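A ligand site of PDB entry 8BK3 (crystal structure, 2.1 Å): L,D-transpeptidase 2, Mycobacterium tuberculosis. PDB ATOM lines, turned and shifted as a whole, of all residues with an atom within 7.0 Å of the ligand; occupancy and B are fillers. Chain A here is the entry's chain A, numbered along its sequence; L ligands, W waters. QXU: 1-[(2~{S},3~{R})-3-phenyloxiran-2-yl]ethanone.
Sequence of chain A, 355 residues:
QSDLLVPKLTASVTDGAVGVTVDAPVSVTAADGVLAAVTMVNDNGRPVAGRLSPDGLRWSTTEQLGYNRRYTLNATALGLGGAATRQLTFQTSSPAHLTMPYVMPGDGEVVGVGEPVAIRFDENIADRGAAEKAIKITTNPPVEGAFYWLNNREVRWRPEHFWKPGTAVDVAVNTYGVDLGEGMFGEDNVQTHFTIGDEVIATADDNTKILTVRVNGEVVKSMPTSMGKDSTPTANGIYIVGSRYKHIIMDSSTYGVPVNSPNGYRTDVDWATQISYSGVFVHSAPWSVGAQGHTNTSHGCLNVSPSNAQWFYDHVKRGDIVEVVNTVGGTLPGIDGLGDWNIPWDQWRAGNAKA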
ATOM      1  N   GLY A 228     -24.233  15.838  18.872  1.00  0.00           N
ATOM      2  CA  GLY A 228     -23.106  16.147  19.742  1.00  0.00           C
ATOM      3  C   GLY A 228     -22.538  14.884  20.367  1.00  0.00           C
ATOM      4  O   GLY A 228     -23.278  13.950  20.705  1.00  0.00           O
ATOM      5  N   THR A 232     -19.969  16.905  24.633  1.00  0.00           N
ATOM      6  CA  THR A 232     -20.805  18.057  24.304  1.00  0.00           C
ATOM      7  C   THR A 232     -22.082  17.572  23.617  1.00  0.00           C
ATOM      8  O   THR A 232     -22.324  17.860  22.440  1.00  0.00           O
ATOM      9  CB  THR A 232     -20.039  19.047  23.414  1.00  0.00           C
ATOM     10  OG1 THR A 232     -19.654  18.383  22.197  1.00  0.00           O
ATOM     11  CG2 THR A 232     -18.793  19.553  24.126  1.00  0.00           C
ATOM     12  N   MET A 250     -20.256  30.003  12.302  1.00  0.00           N
ATOM     13  CA  MET A 250     -20.582  29.472  13.626  1.00  0.00           C
ATOM     14  C   MET A 250     -19.454  29.854  14.565  1.00  0.00           C
ATOM     15  O   MET A 250     -18.390  29.220  14.572  1.00  0.00           O
ATOM     16  CB  MET A 250     -20.767  27.962  13.561  1.00  0.00           C
ATOM     17  CG  MET A 250     -21.732  27.501  12.502  1.00  0.00           C
ATOM     18  SD  MET A 250     -23.436  27.622  13.053  1.00  0.00           S
ATOM     19  CE  MET A 250     -23.581  26.069  13.960  1.00  0.00           C
ATOM     20  N   ASP A 251     -19.670  30.887  15.368  1.00  0.00           N
ATOM     21  CA  ASP A 251     -18.681  31.392  16.305  1.00  0.00           C
ATOM     22  C   ASP A 251     -19.140  31.046  17.716  1.00  0.00           C
ATOM     23  O   ASP A 251     -20.172  31.549  18.180  1.00  0.00           O
ATOM     24  CB  ASP A 251     -18.489  32.896  16.148  1.00  0.00           C
ATOM     25  CG  ASP A 251     -17.375  33.445  17.024  1.00  0.00           C
ATOM     26  OD1 ASP A 251     -16.921  32.724  17.935  1.00  0.00           O
ATOM     27  OD2 ASP A 251     -16.938  34.590  16.784  1.00  0.00           O
ATOM     28  N   TYR A 255     -21.709  32.590  22.167  1.00  0.00           N
ATOM     29  CA  TYR A 255     -22.417  31.829  23.185  1.00  0.00           C
ATOM     30  C   TYR A 255     -21.621  31.734  24.483  1.00  0.00           C
ATOM     31  O   TYR A 255     -21.961  30.933  25.354  1.00  0.00           O
ATOM     32  CB  TYR A 255     -22.740  30.420  22.655  1.00  0.00           C
ATOM     33  CG  TYR A 255     -23.448  30.442  21.319  1.00  0.00           C
ATOM     34  CD1 TYR A 255     -24.818  30.670  21.244  1.00  0.00           C
ATOM     35  CD2 TYR A 255     -22.752  30.238  20.146  1.00  0.00           C
ATOM     36  CE1 TYR A 255     -25.474  30.700  20.023  1.00  0.00           C
ATOM     37  CE2 TYR A 255     -23.400  30.252  18.916  1.00  0.00           C
ATOM     38  CZ  TYR A 255     -24.760  30.496  18.864  1.00  0.00           C
ATOM     39  OH  TYR A 255     -25.407  30.516  17.647  1.00  0.00           O
ATOM     40  N   GLY A 264     -14.491  25.286  22.059  1.00  0.00           N
ATOM     41  CA  GLY A 264     -14.753  26.413  21.187  1.00  0.00           C
ATOM     42  C   GLY A 264     -14.522  26.090  19.729  1.00  0.00           C
ATOM     43  O   GLY A 264     -13.983  25.045  19.366  1.00  0.00           O
ATOM     44  N   TYR A 265     -14.938  27.024  18.870  1.00  0.00           N
ATOM     45  CA  TYR A 265     -14.855  26.816  17.437  1.00  0.00           C
ATOM     46  C   TYR A 265     -15.213  28.103  16.706  1.00  0.00           C
ATOM     47  O   TYR A 265     -15.827  29.005  17.276  1.00  0.00           O
ATOM     48  CB  TYR A 265     -15.791  25.689  16.996  1.00  0.00           C
ATOM     49  CG  TYR A 265     -17.207  25.861  17.521  1.00  0.00           C
ATOM     50  CD1 TYR A 265     -18.126  26.675  16.867  1.00  0.00           C
ATOM     51  CD2 TYR A 265     -17.625  25.221  18.677  1.00  0.00           C
ATOM     52  CE1 TYR A 265     -19.399  26.834  17.339  1.00  0.00           C
ATOM     53  CE2 TYR A 265     -18.901  25.372  19.161  1.00  0.00           C
ATOM     54  CZ  TYR A 265     -19.789  26.186  18.488  1.00  0.00           C
ATOM     55  OH  TYR A 265     -21.070  26.339  18.963  1.00  0.00           O
ATOM     56  N   ARG A 266     -14.814  28.161  15.439  1.00  0.00           N
ATOM     57  CA  ARG A 266     -15.200  29.253  14.547  1.00  0.00           C
ATOM     58  C   ARG A 266     -15.084  28.714  13.131  1.00  0.00           C
ATOM     59  O   ARG A 266     -13.996  28.689  12.557  1.00  0.00           O
ATOM     60  CB  ARG A 266     -14.339  30.481  14.751  1.00  0.00           C
ATOM     61  CG  ARG A 266     -14.722  31.667  13.872  1.00  0.00           C
ATOM     62  CD  ARG A 266     -13.985  32.921  14.362  1.00  0.00           C
ATOM     63  NE  ARG A 266     -12.555  32.673  14.455  1.00  0.00           N
ATOM     64  CZ  ARG A 266     -11.745  33.254  15.329  1.00  0.00           C
ATOM     65  NH1 ARG A 266     -12.227  34.134  16.199  1.00  0.00           N
ATOM     66  NH2 ARG A 266     -10.448  32.953  15.318  1.00  0.00           N
ATOM     67  N   THR A 267     -16.205  28.263  12.577  1.00  0.00           N
ATOM     68  CA  THR A 267     -16.219  27.624  11.270  1.00  0.00           C
ATOM     69  C   THR A 267     -17.428  28.095  10.473  1.00  0.00           C
ATOM     70  O   THR A 267     -18.518  28.273  11.021  1.00  0.00           O
ATOM     71  CB  THR A 267     -16.232  26.092  11.407  1.00  0.00           C
ATOM     72  OG1 THR A 267     -15.100  25.661  12.177  1.00  0.00           O
ATOM     73  CG2 THR A 267     -16.182  25.434  10.032  1.00  0.00           C
ATOM     74  N   ASP A 268     -17.212  28.285   9.174  1.00  0.00           N
ATOM     75  CA  ASP A 268     -18.256  28.728   8.258  1.00  0.00           C
ATOM     76  C   ASP A 268     -18.957  27.503   7.683  1.00  0.00           C
ATOM     77  O   ASP A 268     -18.312  26.675   7.031  1.00  0.00           O
ATOM     78  CB  ASP A 268     -17.665  29.593   7.159  1.00  0.00           C
ATOM     79  CG  ASP A 268     -18.725  30.318   6.347  1.00  0.00           C
ATOM     80  OD1 ASP A 268     -19.940  30.125   6.634  1.00  0.00           O
ATOM     81  OD2 ASP A 268     -18.352  31.063   5.428  1.00  0.00           O
ATOM     82  N   VAL A 269     -20.263  27.403   7.906  1.00  0.00           N
ATOM     83  CA  VAL A 269     -21.056  26.266   7.449  1.00  0.00           C
ATOM     84  C   VAL A 269     -22.140  26.754   6.510  1.00  0.00           C
ATOM     85  O   VAL A 269     -22.474  27.948   6.457  1.00  0.00           O
ATOM     86  CB  VAL A 269     -21.674  25.482   8.623  1.00  0.00           C
ATOM     87  CG1 VAL A 269     -20.608  25.151   9.666  1.00  0.00           C
ATOM     88  CG2 VAL A 269     -22.827  26.264   9.240  1.00  0.00           C
ATOM     89  N   SER A 278     -29.159  28.590  22.225  1.00  0.00           N
ATOM     90  CA  SER A 278     -27.883  28.145  22.750  1.00  0.00           C
ATOM     91  C   SER A 278     -26.891  27.711  21.657  1.00  0.00           C
ATOM     92  O   SER A 278     -25.755  27.359  21.992  1.00  0.00           O
ATOM     93  CB  SER A 278     -28.107  26.980  23.721  1.00  0.00           C
ATOM     94  OG  SER A 278     -28.653  25.855  23.035  1.00  0.00           O
ATOM     95  N   GLY A 279     -27.297  27.724  20.390  1.00  0.00           N
ATOM     96  CA  GLY A 279     -26.395  27.451  19.290  1.00  0.00           C
ATOM     97  C   GLY A 279     -26.569  26.133  18.553  1.00  0.00           C
ATOM     98  O   GLY A 279     -25.655  25.743  17.796  1.00  0.00           O
ATOM     99  N   VAL A 280     -27.686  25.449  18.733  1.00  0.00           N
ATOM    100  CA  VAL A 280     -27.916  24.205  18.015  1.00  0.00           C
ATOM    101  C   VAL A 280     -28.517  24.539  16.659  1.00  0.00           C
ATOM    102  O   VAL A 280     -29.519  25.269  16.558  1.00  0.00           O
ATOM    103  CB  VAL A 280     -28.847  23.275  18.818  1.00  0.00           C
ATOM    104  CG1 VAL A 280     -29.129  22.010  18.029  1.00  0.00           C
ATOM    105  CG2 VAL A 280     -28.226  22.944  20.164  1.00  0.00           C
ATOM    106  N   PHE A 281     -27.897  24.017  15.607  1.00  0.00           N
ATOM    107  CA  PHE A 281     -28.341  24.209  14.235  1.00  0.00           C
ATOM    108  C   PHE A 281     -28.494  22.866  13.538  1.00  0.00           C
ATOM    109  O   PHE A 281     -27.888  21.862  13.939  1.00  0.00           O
ATOM    110  CB  PHE A 281     -27.340  25.068  13.418  1.00  0.00           C
ATOM    111  CG  PHE A 281     -27.330  26.515  13.774  1.00  0.00           C
ATOM    112  CD1 PHE A 281     -26.696  26.968  14.921  1.00  0.00           C
ATOM    113  CD2 PHE A 281     -27.937  27.443  12.942  1.00  0.00           C
ATOM    114  CE1 PHE A 281     -26.669  28.305  15.222  1.00  0.00           C
ATOM    115  CE2 PHE A 281     -27.941  28.780  13.263  1.00  0.00           C
ATOM    116  CZ  PHE A 281     -27.299  29.216  14.399  1.00  0.00           C
ATOM    117  N   HIS A 283     -27.367  21.851   9.924  1.00  0.00           N
ATOM    118  CA  HIS A 283     -26.501  22.480   8.941  1.00  0.00           C
ATOM    119  C   HIS A 283     -25.760  21.427   8.130  1.00  0.00           C
ATOM    120  O   HIS A 283     -25.743  20.241   8.471  1.00  0.00           O
ATOM    121  CB  HIS A 283     -25.484  23.407   9.624  1.00  0.00           C
ATOM    122  CG  HIS A 283     -24.489  22.694  10.490  1.00  0.00           C
ATOM    123  ND1 HIS A 283     -23.250  22.299  10.031  1.00  0.00           N
ATOM    124  CD2 HIS A 283     -24.566  22.280  11.773  1.00  0.00           C
ATOM    125  CE1 HIS A 283     -22.596  21.691  10.999  1.00  0.00           C
ATOM    126  NE2 HIS A 283     -23.375  21.664  12.070  1.00  0.00           N
ATOM    127  N   SER A 284     -25.139  21.889   7.041  1.00  0.00           N
ATOM    128  CA  SER A 284     -24.335  21.021   6.198  1.00  0.00           C
ATOM    129  C   SER A 284     -23.027  20.666   6.898  1.00  0.00           C
ATOM    130  O   SER A 284     -22.367  21.550   7.446  1.00  0.00           O
ATOM    131  CB  SER A 284     -24.055  21.701   4.860  1.00  0.00           C
ATOM    132  OG  SER A 284     -23.159  20.927   4.061  1.00  0.00           O
ATOM    133  N   ALA A 285     -22.667  19.390   6.874  1.00  0.00           N
ATOM    134  CA  ALA A 285     -21.448  18.911   7.519  1.00  0.00           C
ATOM    135  C   ALA A 285     -20.780  17.866   6.634  1.00  0.00           C
ATOM    136  O   ALA A 285     -20.898  16.659   6.857  1.00  0.00           O
ATOM    137  CB  ALA A 285     -21.754  18.331   8.902  1.00  0.00           C
ATOM    138  N   TRP A 287     -17.664  17.096   6.491  1.00  0.00           N
ATOM    139  CA  TRP A 287     -16.558  16.426   7.159  1.00  0.00           C
ATOM    140  C   TRP A 287     -17.006  15.218   7.976  1.00  0.00           C
ATOM    141  O   TRP A 287     -16.173  14.378   8.302  1.00  0.00           O
ATOM    142  CB  TRP A 287     -15.826  17.416   8.080  1.00  0.00           C
ATOM    143  CG  TRP A 287     -16.740  18.060   9.091  1.00  0.00           C
ATOM    144  CD1 TRP A 287     -17.075  17.564  10.324  1.00  0.00           C
ATOM    145  CD2 TRP A 287     -17.448  19.301   8.952  1.00  0.00           C
ATOM    146  NE1 TRP A 287     -17.942  18.416  10.947  1.00  0.00           N
ATOM    147  CE2 TRP A 287     -18.179  19.491  10.141  1.00  0.00           C
ATOM    148  CE3 TRP A 287     -17.527  20.256   7.944  1.00  0.00           C
ATOM    149  CZ2 TRP A 287     -18.991  20.613  10.341  1.00  0.00           C
ATOM    150  CZ3 TRP A 287     -18.321  21.378   8.158  1.00  0.00           C
ATOM    151  CH2 TRP A 287     -19.040  21.544   9.334  1.00  0.00           C
ATOM    152  N   THR A 297     -20.247  13.343  16.720  1.00  0.00           N
ATOM    153  CA  THR A 297     -18.961  14.007  16.673  1.00  0.00           C
ATOM    154  C   THR A 297     -19.021  15.532  16.794  1.00  0.00           C
ATOM    155  O   THR A 297     -17.965  16.163  16.851  1.00  0.00           O
ATOM    156  CB  THR A 297     -18.217  13.642  15.365  1.00  0.00           C
ATOM    157  OG1 THR A 297     -19.038  13.977  14.236  1.00  0.00           O
ATOM    158  CG2 THR A 297     -17.892  12.164  15.316  1.00  0.00           C
ATOM    159  N   SER A 298     -20.202  16.127  16.845  1.00  0.00           N
ATOM    160  CA  SER A 298     -20.296  17.576  16.808  1.00  0.00           C
ATOM    161  C   SER A 298     -20.319  18.147  18.225  1.00  0.00           C
ATOM    162  O   SER A 298     -20.092  17.440  19.205  1.00  0.00           O
ATOM    163  CB  SER A 298     -21.547  18.012  16.038  1.00  0.00           C
ATOM    164  OG  SER A 298     -22.728  17.860  16.844  1.00  0.00           O
ATOM    165  N   HIS A 299     -20.573  19.447  18.336  1.00  0.00           N
ATOM    166  CA  HIS A 299     -20.647  20.130  19.625  1.00  0.00           C
ATOM    167  C   HIS A 299     -22.076  20.262  20.146  1.00  0.00           C
ATOM    168  O   HIS A 299     -22.279  20.828  21.226  1.00  0.00           O
ATOM    169  CB  HIS A 299     -20.026  21.524  19.516  1.00  0.00           C
ATOM    170  CG  HIS A 299     -18.571  21.505  19.168  1.00  0.00           C
ATOM    171  ND1 HIS A 299     -18.108  21.118  17.925  1.00  0.00           N
ATOM    172  CD2 HIS A 299     -17.476  21.848  19.887  1.00  0.00           C
ATOM    173  CE1 HIS A 299     -16.790  21.206  17.907  1.00  0.00           C
ATOM    174  NE2 HIS A 299     -16.379  21.662  19.080  1.00  0.00           N
ATOM    175  N   GLY A 300     -23.059  19.763  19.399  1.00  0.00           N
ATOM    176  CA  GLY A 300     -24.444  19.898  19.775  1.00  0.00           C
ATOM    177  C   GLY A 300     -25.342  20.006  18.566  1.00  0.00           C
ATOM    178  O   GLY A 300     -26.506  19.610  18.618  1.00  0.00           O
ATOM    179  N   CYS A 301     -24.792  20.533  17.477  1.00  0.00           N
ATOM    180  CA  CYS A 301     -25.571  20.737  16.285  1.00  0.00           C
ATOM    181  C   CYS A 301     -25.915  19.403  15.609  1.00  0.00           C
ATOM    182  O   CYS A 301     -25.227  18.443  15.806  1.00  0.00           O
ATOM    183  CB  CYS A 301     -24.794  21.542  15.226  1.00  0.00           C
ATOM    184  SG  CYS A 301     -24.730  23.317  15.622  1.00  0.00           S
ATOM    185  N   LEU A 302     -26.981  19.385  14.825  1.00  0.00           N
ATOM    186  CA  LEU A 302     -27.381  18.218  14.074  1.00  0.00           C
ATOM    187  C   LEU A 302     -26.715  18.269  12.693  1.00  0.00           C
ATOM    188  O   LEU A 302     -27.181  18.950  11.777  1.00  0.00           O
ATOM    189  CB  LEU A 302     -28.901  18.161  13.958  1.00  0.00           C
ATOM    190  CG  LEU A 302     -29.613  17.487  15.124  1.00  0.00           C
ATOM    191  CD1 LEU A 302     -29.165  18.085  16.449  1.00  0.00           C
ATOM    192  CD2 LEU A 302     -31.133  17.606  14.963  1.00  0.00           C
ATOM    193  N   ASN A 303     -25.614  17.537  12.554  1.00  0.00           N
ATOM    194  CA  ASN A 303     -24.898  17.487  11.282  1.00  0.00           C
ATOM    195  C   ASN A 303     -25.655  16.607  10.301  1.00  0.00           C
ATOM    196  O   ASN A 303     -26.042  15.481  10.636  1.00  0.00           O
ATOM    197  CB  ASN A 303     -23.482  16.965  11.472  1.00  0.00           C
ATOM    198  CG  ASN A 303     -22.598  17.938  12.224  1.00  0.00           C
ATOM    199  OD1 ASN A 303     -22.970  19.102  12.474  1.00  0.00           O
ATOM    200  ND2 ASN A 303     -21.420  17.467  12.583  1.00  0.00           N
HETATM  201  C10 QXU L   1     -17.775  22.890  12.309  1.00  0.00           C
HETATM  202  C02 QXU L   1     -22.262  22.728  16.340  1.00  0.00           C
HETATM  203  C03 QXU L   1     -21.641  23.078  14.989  1.00  0.00           C
HETATM  204  C05 QXU L   1     -20.243  23.417  15.165  1.00  0.00           C
HETATM  205  C06 QXU L   1     -18.925  23.227  14.393  1.00  0.00           C
HETATM  206  C07 QXU L   1     -17.704  23.225  15.079  1.00  0.00           C
HETATM  207  C08 QXU L   1     -16.510  23.051  14.374  1.00  0.00           C
HETATM  208  C09 QXU L   1     -16.555  22.883  12.982  1.00  0.00           C
HETATM  209  C11 QXU L   1     -18.965  23.057  13.009  1.00  0.00           C
HETATM  210  C12 QXU L   1     -23.420  23.620  16.848  1.00  0.00           C
HETATM  211  O01 QXU L   1     -21.870  21.784  16.959  1.00  0.00           O
HETATM  212  O04 QXU L   1     -21.149  24.394  14.671  1.00  0.00           O
HETATM  213  O   HOH W   1     -14.924  21.032  10.889  1.00  0.00           O
HETATM  214  O   HOH W   2     -19.055  20.041  14.574  1.00  0.00           O
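O01 of the ligand is in hydrogen-bond range of N of Cys 301 (3.2 Å). SG of Cys 301 is bonded to C12 of the ligand, at 1.8 Å. N of His 299 lies within hydrogen-bond range of O01 of the ligand. The backbone NH of Gly 300 lies within hydrogen-bond range of an oxygen (O01) of the ligand.
The side-chain hydroxyl (OG) of Ser 298 sits at hydrogen-bond distance from the backbone carbonyl oxygen (O) of Cys 301 (2.8 Å). The backbone NH (N) of Phe 281 lies within hydrogen-bond range of the side-chain sulfur (SG) of Cys 301 (3.2 Å). N of Met 250 lies within hydrogen-bond range of O of Thr 267 (2.8 Å). The side-chain hydroxyl (OG) of Ser 298 is in hydrogen-bond range of the backbone NH (N) of Gly 300 (3.2 Å). A ring nitrogen (NE2) of His 283 is in hydrogen-bond range of the side-chain amide oxygen of Asn 303, at 2.6 Å. The backbone NH (N) of His 283 sits at hydrogen-bond distance from the backbone carbonyl oxygen (O) of Leu 302 (3.4 Å). The side-chain hydroxyl of Ser 298 lies within hydrogen-bond range of the backbone NH of Gly 228, at 3.2 Å. O of Ser 298 sits at hydrogen-bond distance from OG1 of Thr 232, 3.2 Å away.
Met 250 touches the ligand. Tyr 265 touches the ligand (CG to C07, 3.6 Å). Thr 267 touches the ligand. Gly 279 touches the ligand. His 283 touches the ligand (NE2 to C03, 3.7 Å). CZ2 of Trp 287 touches C10 of the ligand, at 3.2 Å. CB of Ser 298 touches O01 of the ligand (3.9 Å). Hydrophobic or aromatic side chains that line the ligand: Met 250, Tyr 265, Trp 287 and His 299.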
